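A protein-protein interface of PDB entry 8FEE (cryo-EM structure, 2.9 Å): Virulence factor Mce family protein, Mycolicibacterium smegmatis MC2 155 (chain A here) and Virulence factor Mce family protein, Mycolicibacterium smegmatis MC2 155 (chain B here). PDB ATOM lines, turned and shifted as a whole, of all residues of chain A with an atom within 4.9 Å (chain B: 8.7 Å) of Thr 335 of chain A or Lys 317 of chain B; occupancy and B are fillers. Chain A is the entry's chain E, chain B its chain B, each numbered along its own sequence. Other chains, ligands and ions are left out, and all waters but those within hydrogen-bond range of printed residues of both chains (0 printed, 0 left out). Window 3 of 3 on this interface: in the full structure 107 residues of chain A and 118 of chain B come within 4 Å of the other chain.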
ATOM      1  N   LYS A 331      -2.557   9.273 -26.179  1.00  0.00           N
ATOM      2  CA  LYS A 331      -3.597   8.648 -25.366  1.00  0.00           C
ATOM      3  C   LYS A 331      -4.158   9.741 -24.458  1.00  0.00           C
ATOM      4  O   LYS A 331      -3.680   9.954 -23.343  1.00  0.00           O
ATOM      5  CB  LYS A 331      -3.039   7.468 -24.564  1.00  0.00           C
ATOM      6  CG  LYS A 331      -4.011   6.864 -23.560  1.00  0.00           C
ATOM      7  CD  LYS A 331      -4.574   5.543 -24.040  1.00  0.00           C
ATOM      8  CE  LYS A 331      -3.543   4.435 -23.920  1.00  0.00           C
ATOM      9  NZ  LYS A 331      -4.133   3.098 -24.207  1.00  0.00           N
ATOM     10  N   LEU A 332      -5.164  10.459 -24.961  1.00  0.00           N
ATOM     11  CA  LEU A 332      -5.807  11.528 -24.197  1.00  0.00           C
ATOM     12  C   LEU A 332      -6.673  10.898 -23.111  1.00  0.00           C
ATOM     13  O   LEU A 332      -7.881  10.702 -23.264  1.00  0.00           O
ATOM     14  CB  LEU A 332      -6.634  12.435 -25.103  1.00  0.00           C
ATOM     15  CG  LEU A 332      -5.931  13.394 -26.069  1.00  0.00           C
ATOM     16  CD1 LEU A 332      -5.426  12.685 -27.318  1.00  0.00           C
ATOM     17  CD2 LEU A 332      -6.857  14.541 -26.441  1.00  0.00           C
ATOM     18  N   ASP A 333      -6.041  10.579 -21.985  1.00  0.00           N
ATOM     19  CA  ASP A 333      -6.721   9.830 -20.936  1.00  0.00           C
ATOM     20  C   ASP A 333      -7.529  10.785 -20.063  1.00  0.00           C
ATOM     21  O   ASP A 333      -6.975  11.698 -19.442  1.00  0.00           O
ATOM     22  CB  ASP A 333      -5.720   9.019 -20.111  1.00  0.00           C
ATOM     23  CG  ASP A 333      -4.686   9.882 -19.426  1.00  0.00           C
ATOM     24  OD1 ASP A 333      -4.235  10.869 -20.041  1.00  0.00           O
ATOM     25  OD2 ASP A 333      -4.327   9.574 -18.271  1.00  0.00           O
ATOM     26  N   LEU A 334      -8.844  10.589 -20.042  1.00  0.00           N
ATOM     27  CA  LEU A 334      -9.759  11.371 -19.219  1.00  0.00           C
ATOM     28  C   LEU A 334     -10.269  10.557 -18.033  1.00  0.00           C
ATOM     29  O   LEU A 334     -11.423  10.684 -17.620  1.00  0.00           O
ATOM     30  CB  LEU A 334     -10.922  11.893 -20.057  1.00  0.00           C
ATOM     31  CG  LEU A 334     -10.540  12.567 -21.376  1.00  0.00           C
ATOM     32  CD1 LEU A 334     -11.775  13.073 -22.101  1.00  0.00           C
ATOM     33  CD2 LEU A 334      -9.558  13.702 -21.135  1.00  0.00           C
ATOM     34  N   THR A 335      -9.410   9.705 -17.482  1.00  0.00           N
ATOM     35  CA  THR A 335      -9.762   8.920 -16.311  1.00  0.00           C
ATOM     36  C   THR A 335      -9.985   9.837 -15.108  1.00  0.00           C
ATOM     37  O   THR A 335      -9.470  10.957 -15.044  1.00  0.00           O
ATOM     38  CB  THR A 335      -8.654   7.903 -16.012  1.00  0.00           C
ATOM     39  OG1 THR A 335      -8.159   7.367 -17.245  1.00  0.00           O
ATOM     40  CG2 THR A 335      -9.175   6.754 -15.165  1.00  0.00           C
ATOM     41  N   LEU A 336     -10.786   9.354 -14.153  1.00  0.00           N
ATOM     42  CA  LEU A 336     -11.082  10.147 -12.963  1.00  0.00           C
ATOM     43  C   LEU A 336      -9.822  10.422 -12.153  1.00  0.00           C
ATOM     44  O   LEU A 336      -9.615  11.543 -11.678  1.00  0.00           O
ATOM     45  CB  LEU A 336     -12.132   9.444 -12.101  1.00  0.00           C
ATOM     46  CG  LEU A 336     -13.574   9.457 -12.611  1.00  0.00           C
ATOM     47  CD1 LEU A 336     -14.513   8.871 -11.569  1.00  0.00           C
ATOM     48  CD2 LEU A 336     -14.007  10.863 -12.996  1.00  0.00           C
ATOM     49  N   SER A 337      -8.970   9.407 -11.979  1.00  0.00           N
ATOM     50  CA  SER A 337      -7.743   9.593 -11.210  1.00  0.00           C
ATOM     51  C   SER A 337      -6.780  10.539 -11.917  1.00  0.00           C
ATOM     52  O   SER A 337      -6.101  11.343 -11.267  1.00  0.00           O
ATOM     53  CB  SER A 337      -7.073   8.244 -10.956  1.00  0.00           C
ATOM     54  OG  SER A 337      -6.683   7.632 -12.171  1.00  0.00           O
ATOM     55  N   SER A 338      -6.699  10.448 -13.247  1.00  0.00           N
ATOM     56  CA  SER A 338      -5.821  11.337 -14.000  1.00  0.00           C
ATOM     57  C   SER A 338      -6.257  12.792 -13.868  1.00  0.00           C
ATOM     58  O   SER A 338      -5.421  13.682 -13.676  1.00  0.00           O
ATOM     59  CB  SER A 338      -5.787  10.920 -15.470  1.00  0.00           C
ATOM     60  OG  SER A 338      -7.054  11.096 -16.078  1.00  0.00           O
ATOM     61  N   VAL A 339      -7.562  13.051 -13.963  1.00  0.00           N
ATOM     62  CA  VAL A 339      -8.066  14.413 -13.808  1.00  0.00           C
ATOM     63  C   VAL A 339      -7.910  14.880 -12.364  1.00  0.00           C
ATOM     64  O   VAL A 339      -7.622  16.055 -12.104  1.00  0.00           O
ATOM     65  CB  VAL A 339      -9.528  14.489 -14.287  1.00  0.00           C
ATOM     66  CG1 VAL A 339     -10.165  15.817 -13.907  1.00  0.00           C
ATOM     67  CG2 VAL A 339      -9.597  14.282 -15.791  1.00  0.00           C
ATOM     68  N   GLU A 357     -13.998   6.633  -8.020  1.00  0.00           N
ATOM     69  CA  GLU A 357     -13.593   5.607  -8.974  1.00  0.00           C
ATOM     70  C   GLU A 357     -13.029   4.376  -8.278  1.00  0.00           C
ATOM     71  O   GLU A 357     -13.116   3.270  -8.822  1.00  0.00           O
ATOM     72  CB  GLU A 357     -12.563   6.161  -9.957  1.00  0.00           C
ATOM     73  CG  GLU A 357     -12.444   5.331 -11.222  1.00  0.00           C
ATOM     74  CD  GLU A 357     -11.490   5.923 -12.237  1.00  0.00           C
ATOM     75  OE1 GLU A 357     -10.585   6.684 -11.837  1.00  0.00           O
ATOM     76  OE2 GLU A 357     -11.649   5.626 -13.439  1.00  0.00           O
ATOM     77  N   ARG A 362     -12.427  -0.189 -10.660  1.00  0.00           N
ATOM     78  CA  ARG A 362     -11.016   0.158 -10.751  1.00  0.00           C
ATOM     79  C   ARG A 362     -10.264  -0.333  -9.519  1.00  0.00           C
ATOM     80  O   ARG A 362     -10.802  -0.380  -8.410  1.00  0.00           O
ATOM     81  CB  ARG A 362     -10.847   1.669 -10.907  1.00  0.00           C
ATOM     82  CG  ARG A 362     -11.080   2.164 -12.325  1.00  0.00           C
ATOM     83  CD  ARG A 362      -9.854   1.966 -13.204  1.00  0.00           C
ATOM     84  NE  ARG A 362      -8.940   3.099 -13.126  1.00  0.00           N
ATOM     85  CZ  ARG A 362      -7.828   3.216 -13.838  1.00  0.00           C
ATOM     86  NH1 ARG A 362      -7.439   2.268 -14.674  1.00  0.00           N
ATOM     87  NH2 ARG A 362      -7.085   4.312 -13.707  1.00  0.00           N
ATOM     88  N   LEU B 314      -4.167   8.647 -32.802  1.00  0.00           N
ATOM     89  CA  LEU B 314      -4.564   9.190 -31.511  1.00  0.00           C
ATOM     90  C   LEU B 314      -5.742   8.401 -30.958  1.00  0.00           C
ATOM     91  O   LEU B 314      -6.629   7.984 -31.708  1.00  0.00           O
ATOM     92  CB  LEU B 314      -4.916  10.684 -31.617  1.00  0.00           C
ATOM     93  CG  LEU B 314      -6.056  11.117 -32.539  1.00  0.00           C
ATOM     94  CD1 LEU B 314      -7.306  11.423 -31.733  1.00  0.00           C
ATOM     95  CD2 LEU B 314      -5.643  12.323 -33.365  1.00  0.00           C
ATOM     96  N   THR B 315      -5.740   8.197 -29.644  1.00  0.00           N
ATOM     97  CA  THR B 315      -6.794   7.465 -28.961  1.00  0.00           C
ATOM     98  C   THR B 315      -7.240   8.245 -27.733  1.00  0.00           C
ATOM     99  O   THR B 315      -6.492   9.054 -27.179  1.00  0.00           O
ATOM    100  CB  THR B 315      -6.338   6.058 -28.547  1.00  0.00           C
ATOM    101  OG1 THR B 315      -7.314   5.473 -27.677  1.00  0.00           O
ATOM    102  CG2 THR B 315      -5.004   6.121 -27.827  1.00  0.00           C
ATOM    103  N   LEU B 316      -8.476   7.993 -27.313  1.00  0.00           N
ATOM    104  CA  LEU B 316      -9.040   8.582 -26.106  1.00  0.00           C
ATOM    105  C   LEU B 316      -9.279   7.487 -25.078  1.00  0.00           C
ATOM    106  O   LEU B 316      -9.846   6.439 -25.403  1.00  0.00           O
ATOM    107  CB  LEU B 316     -10.348   9.321 -26.401  1.00  0.00           C
ATOM    108  CG  LEU B 316     -10.282  10.754 -26.937  1.00  0.00           C
ATOM    109  CD1 LEU B 316      -9.699  10.815 -28.339  1.00  0.00           C
ATOM    110  CD2 LEU B 316     -11.659  11.397 -26.903  1.00  0.00           C
ATOM    111  N   LYS B 317      -8.845   7.730 -23.847  1.00  0.00           N
ATOM    112  CA  LYS B 317      -9.055   6.816 -22.735  1.00  0.00           C
ATOM    113  C   LYS B 317      -9.958   7.491 -21.715  1.00  0.00           C
ATOM    114  O   LYS B 317      -9.694   8.628 -21.309  1.00  0.00           O
ATOM    115  CB  LYS B 317      -7.724   6.412 -22.098  1.00  0.00           C
ATOM    116  CG  LYS B 317      -7.853   5.525 -20.876  1.00  0.00           C
ATOM    117  CD  LYS B 317      -6.486   5.213 -20.293  1.00  0.00           C
ATOM    118  CE  LYS B 317      -6.580   4.234 -19.138  1.00  0.00           C
ATOM    119  NZ  LYS B 317      -5.235   3.880 -18.615  1.00  0.00           N
ATOM    120  N   LEU B 318     -11.015   6.800 -21.306  1.00  0.00           N
ATOM    121  CA  LEU B 318     -11.988   7.354 -20.370  1.00  0.00           C
ATOM    122  C   LEU B 318     -12.824   6.208 -19.812  1.00  0.00           C
ATOM    123  O   LEU B 318     -12.555   5.033 -20.081  1.00  0.00           O
ATOM    124  CB  LEU B 318     -12.849   8.427 -21.049  1.00  0.00           C
ATOM    125  CG  LEU B 318     -13.567   8.089 -22.360  1.00  0.00           C
ATOM    126  CD1 LEU B 318     -14.959   7.524 -22.116  1.00  0.00           C
ATOM    127  CD2 LEU B 318     -13.634   9.311 -23.259  1.00  0.00           C
ATOM    128  N   ASN B 319     -13.840   6.553 -19.028  1.00  0.00           N
ATOM    129  CA  ASN B 319     -14.751   5.564 -18.466  1.00  0.00           C
ATOM    130  C   ASN B 319     -16.183   6.090 -18.422  1.00  0.00           C
ATOM    131  O   ASN B 319     -16.787   6.362 -19.460  1.00  0.00           O
ATOM    132  CB  ASN B 319     -14.295   5.150 -17.063  1.00  0.00           C
ATOM    133  CG  ASN B 319     -13.951   6.336 -16.185  1.00  0.00           C
ATOM    134  OD1 ASN B 319     -14.302   7.475 -16.489  1.00  0.00           O
ATOM    135  ND2 ASN B 319     -13.258   6.072 -15.085  1.00  0.00           N
ATOM    136  N   VAL B 327     -13.690   2.237 -18.607  1.00  0.00           N
ATOM    137  CA  VAL B 327     -12.272   2.014 -18.846  1.00  0.00           C
ATOM    138  C   VAL B 327     -12.056   1.799 -20.344  1.00  0.00           C
ATOM    139  O   VAL B 327     -10.942   1.533 -20.799  1.00  0.00           O
ATOM    140  CB  VAL B 327     -11.752   0.823 -18.009  1.00  0.00           C
ATOM    141  CG1 VAL B 327     -12.147  -0.506 -18.645  1.00  0.00           C
ATOM    142  CG2 VAL B 327     -10.243   0.921 -17.786  1.00  0.00           C
ATOM    143  N   ARG B 328     -13.136   1.943 -21.108  1.00  0.00           N
ATOM    144  CA  ARG B 328     -13.078   1.749 -22.549  1.00  0.00           C
ATOM    145  C   ARG B 328     -12.214   2.817 -23.212  1.00  0.00           C
ATOM    146  O   ARG B 328     -12.142   3.964 -22.762  1.00  0.00           O
ATOM    147  CB  ARG B 328     -14.485   1.777 -23.148  1.00  0.00           C
ATOM    148  CG  ARG B 328     -15.241   3.070 -22.893  1.00  0.00           C
ATOM    149  CD  ARG B 328     -16.408   3.225 -23.852  1.00  0.00           C
ATOM    150  NE  ARG B 328     -16.931   4.586 -23.862  1.00  0.00           N
ATOM    151  CZ  ARG B 328     -17.736   5.073 -24.796  1.00  0.00           C
ATOM    152  NH1 ARG B 328     -18.131   4.336 -25.821  1.00  0.00           N
ATOM    153  NH2 ARG B 328     -18.152   6.332 -24.701  1.00  0.00           N
ATOM    154  N   THR B 329     -11.548   2.423 -24.294  1.00  0.00           N
ATOM    155  CA  THR B 329     -10.685   3.309 -25.062  1.00  0.00           C
ATOM    156  C   THR B 329     -11.289   3.524 -26.443  1.00  0.00           C
ATOM    157  O   THR B 329     -11.625   2.557 -27.133  1.00  0.00           O
ATOM    158  CB  THR B 329      -9.273   2.732 -25.185  1.00  0.00           C
ATOM    159  OG1 THR B 329      -9.321   1.497 -25.911  1.00  0.00           O
ATOM    160  CG2 THR B 329      -8.680   2.476 -23.806  1.00  0.00           C
ATOM    161  N   VAL B 330     -11.421   4.786 -26.844  1.00  0.00           N
ATOM    162  CA  VAL B 330     -12.072   5.154 -28.096  1.00  0.00           C
ATOM    163  C   VAL B 330     -11.032   5.763 -29.024  1.00  0.00           C
ATOM    164  O   VAL B 330     -10.327   6.707 -28.647  1.00  0.00           O
ATOM    165  CB  VAL B 330     -13.237   6.131 -27.859  1.00  0.00           C
ATOM    166  CG1 VAL B 330     -13.787   6.636 -29.185  1.00  0.00           C
ATOM    167  CG2 VAL B 330     -14.329   5.462 -27.041  1.00  0.00           C
ATOM    168  N   ARG B 331     -10.944   5.228 -30.238  1.00  0.00           N
ATOM    169  CA  ARG B 331     -10.002   5.692 -31.246  1.00  0.00           C
ATOM    170  C   ARG B 331     -10.710   6.598 -32.245  1.00  0.00           C
ATOM    171  O   ARG B 331     -11.829   6.308 -32.676  1.00  0.00           O
ATOM    172  CB  ARG B 331      -9.361   4.498 -31.962  1.00  0.00           C
ATOM    173  CG  ARG B 331      -8.608   4.828 -33.243  1.00  0.00           C
ATOM    174  CD  ARG B 331      -9.405   4.470 -34.500  1.00  0.00           C
ATOM    175  NE  ARG B 331      -9.692   3.043 -34.592  1.00  0.00           N
ATOM    176  CZ  ARG B 331     -10.869   2.493 -34.322  1.00  0.00           C
ATOM    177  NH1 ARG B 331     -11.902   3.223 -33.937  1.00  0.00           N
ATOM    178  NH2 ARG B 331     -11.012   1.176 -34.442  1.00  0.00           N
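N of Leu 332 of chain A is in hydrogen-bond range of O of Thr 315 of chain B (2.9 Å).
The backbone carbonyl oxygen of Leu 332 of chain A lies within hydrogen-bond range of the backbone NH of Lys 317 of chain B (3.2 Å).
N of Leu 334 of chain A lies within hydrogen-bond range of O of Lys 317 of chain B (2.5 Å).
OE2 of Glu 357 of chain A lies close to ND2 of Asn 319 of chain B (2.3 Å).
The backbone carbonyl oxygen (O) of Val 330 of chain B is in hydrogen-bond range of the side-chain hydroxyl (OG1) of Thr 315 of chain B.
The backbone NH of Leu 316 of chain B is in hydrogen-bond range of the backbone carbonyl oxygen of Val 330 of chain B (2.6 Å).
OG of Ser 338 of chain A is in hydrogen-bond range of O of Asp 333 of chain A, 3.4 Å away.
The backbone carbonyl oxygen (O) of Thr 335 of chain A is in hydrogen-bond range of the side-chain hydroxyl (OG) of Ser 338 of chain A, 2.6 Å away.
The backbone NH (N) of Ser 337 of chain A lies within hydrogen-bond range of the side-chain carboxylate (OE1) of Glu 357 of chain A (3.2 Å).
The guanidinium group of Arg 362 of chain A lies within salt-bridge range of the side-chain carboxylate of Glu 357 of chain A.
Among the printed residues, merely in contact across the chains: Lys 331 of chain A with Thr 315 of chain B (3.4 Å), Lys 331 of chain A with Lys 317 of chain B (3.8 Å), Leu 332 of chain A with Leu 316 of chain B (3.7 Å), Asp 333 of chain A with Lys 317 of chain B (3.2 Å) and Thr 335 of chain A with Lys 317 of chain B (3.99 Å).
Printed residues of chain B within 4 Å of Leu 332 of chain A: Thr 315 (2.9 Å), Leu 316 (3.7 Å) and Lys 317 (3.2 Å).
Printed residues of chain B within 4 Å of Leu 334 of chain A: Lys 317 (2.5 Å).
Printed residues of chain B within 4 Å of Thr 335 of chain A: Lys 317 (3.99 Å).
Ser 338 of chain A touches none of the printed residues of chain B.
Printed residues of chain B within 4 Å of Glu 357 of chain A: Asn 319.
Of the printed residues of chain A, Lys 317 of chain B touches Lys 331, Leu 332, Asp 333, Leu 334 and Thr 335.
Leu 318 of chain B touches none of the printed residues of chain A.
The nearest printed residue of chain B that does not touch Thr 335 of chain A is Asn 319 of chain B (4.1 Å).
The nearest printed residue of chain A that does not touch Lys 317 of chain B is Arg 362 of chain A (4.8 Å).
Of the 11 printed residues of chain A, 6 touch a printed residue of chain B.
Hydrophobic or aromatic side chains of chain A that line the printed part of chain B: Leu 332 and Leu 334.
Printed residues of chain B that touch a printed residue of chain A: Thr 315, Leu 316, Lys 317 and Asn 319.
Along chain B the printed residues that touch a printed residue of chain A span positions 315 to 319.
Among the printed residues, 9 pairs touch across the chains.
Among the printed residues, no Asp or Glu carboxylate lies within 4 Å of a Lys or Arg side-chain nitrogen of the other chain.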
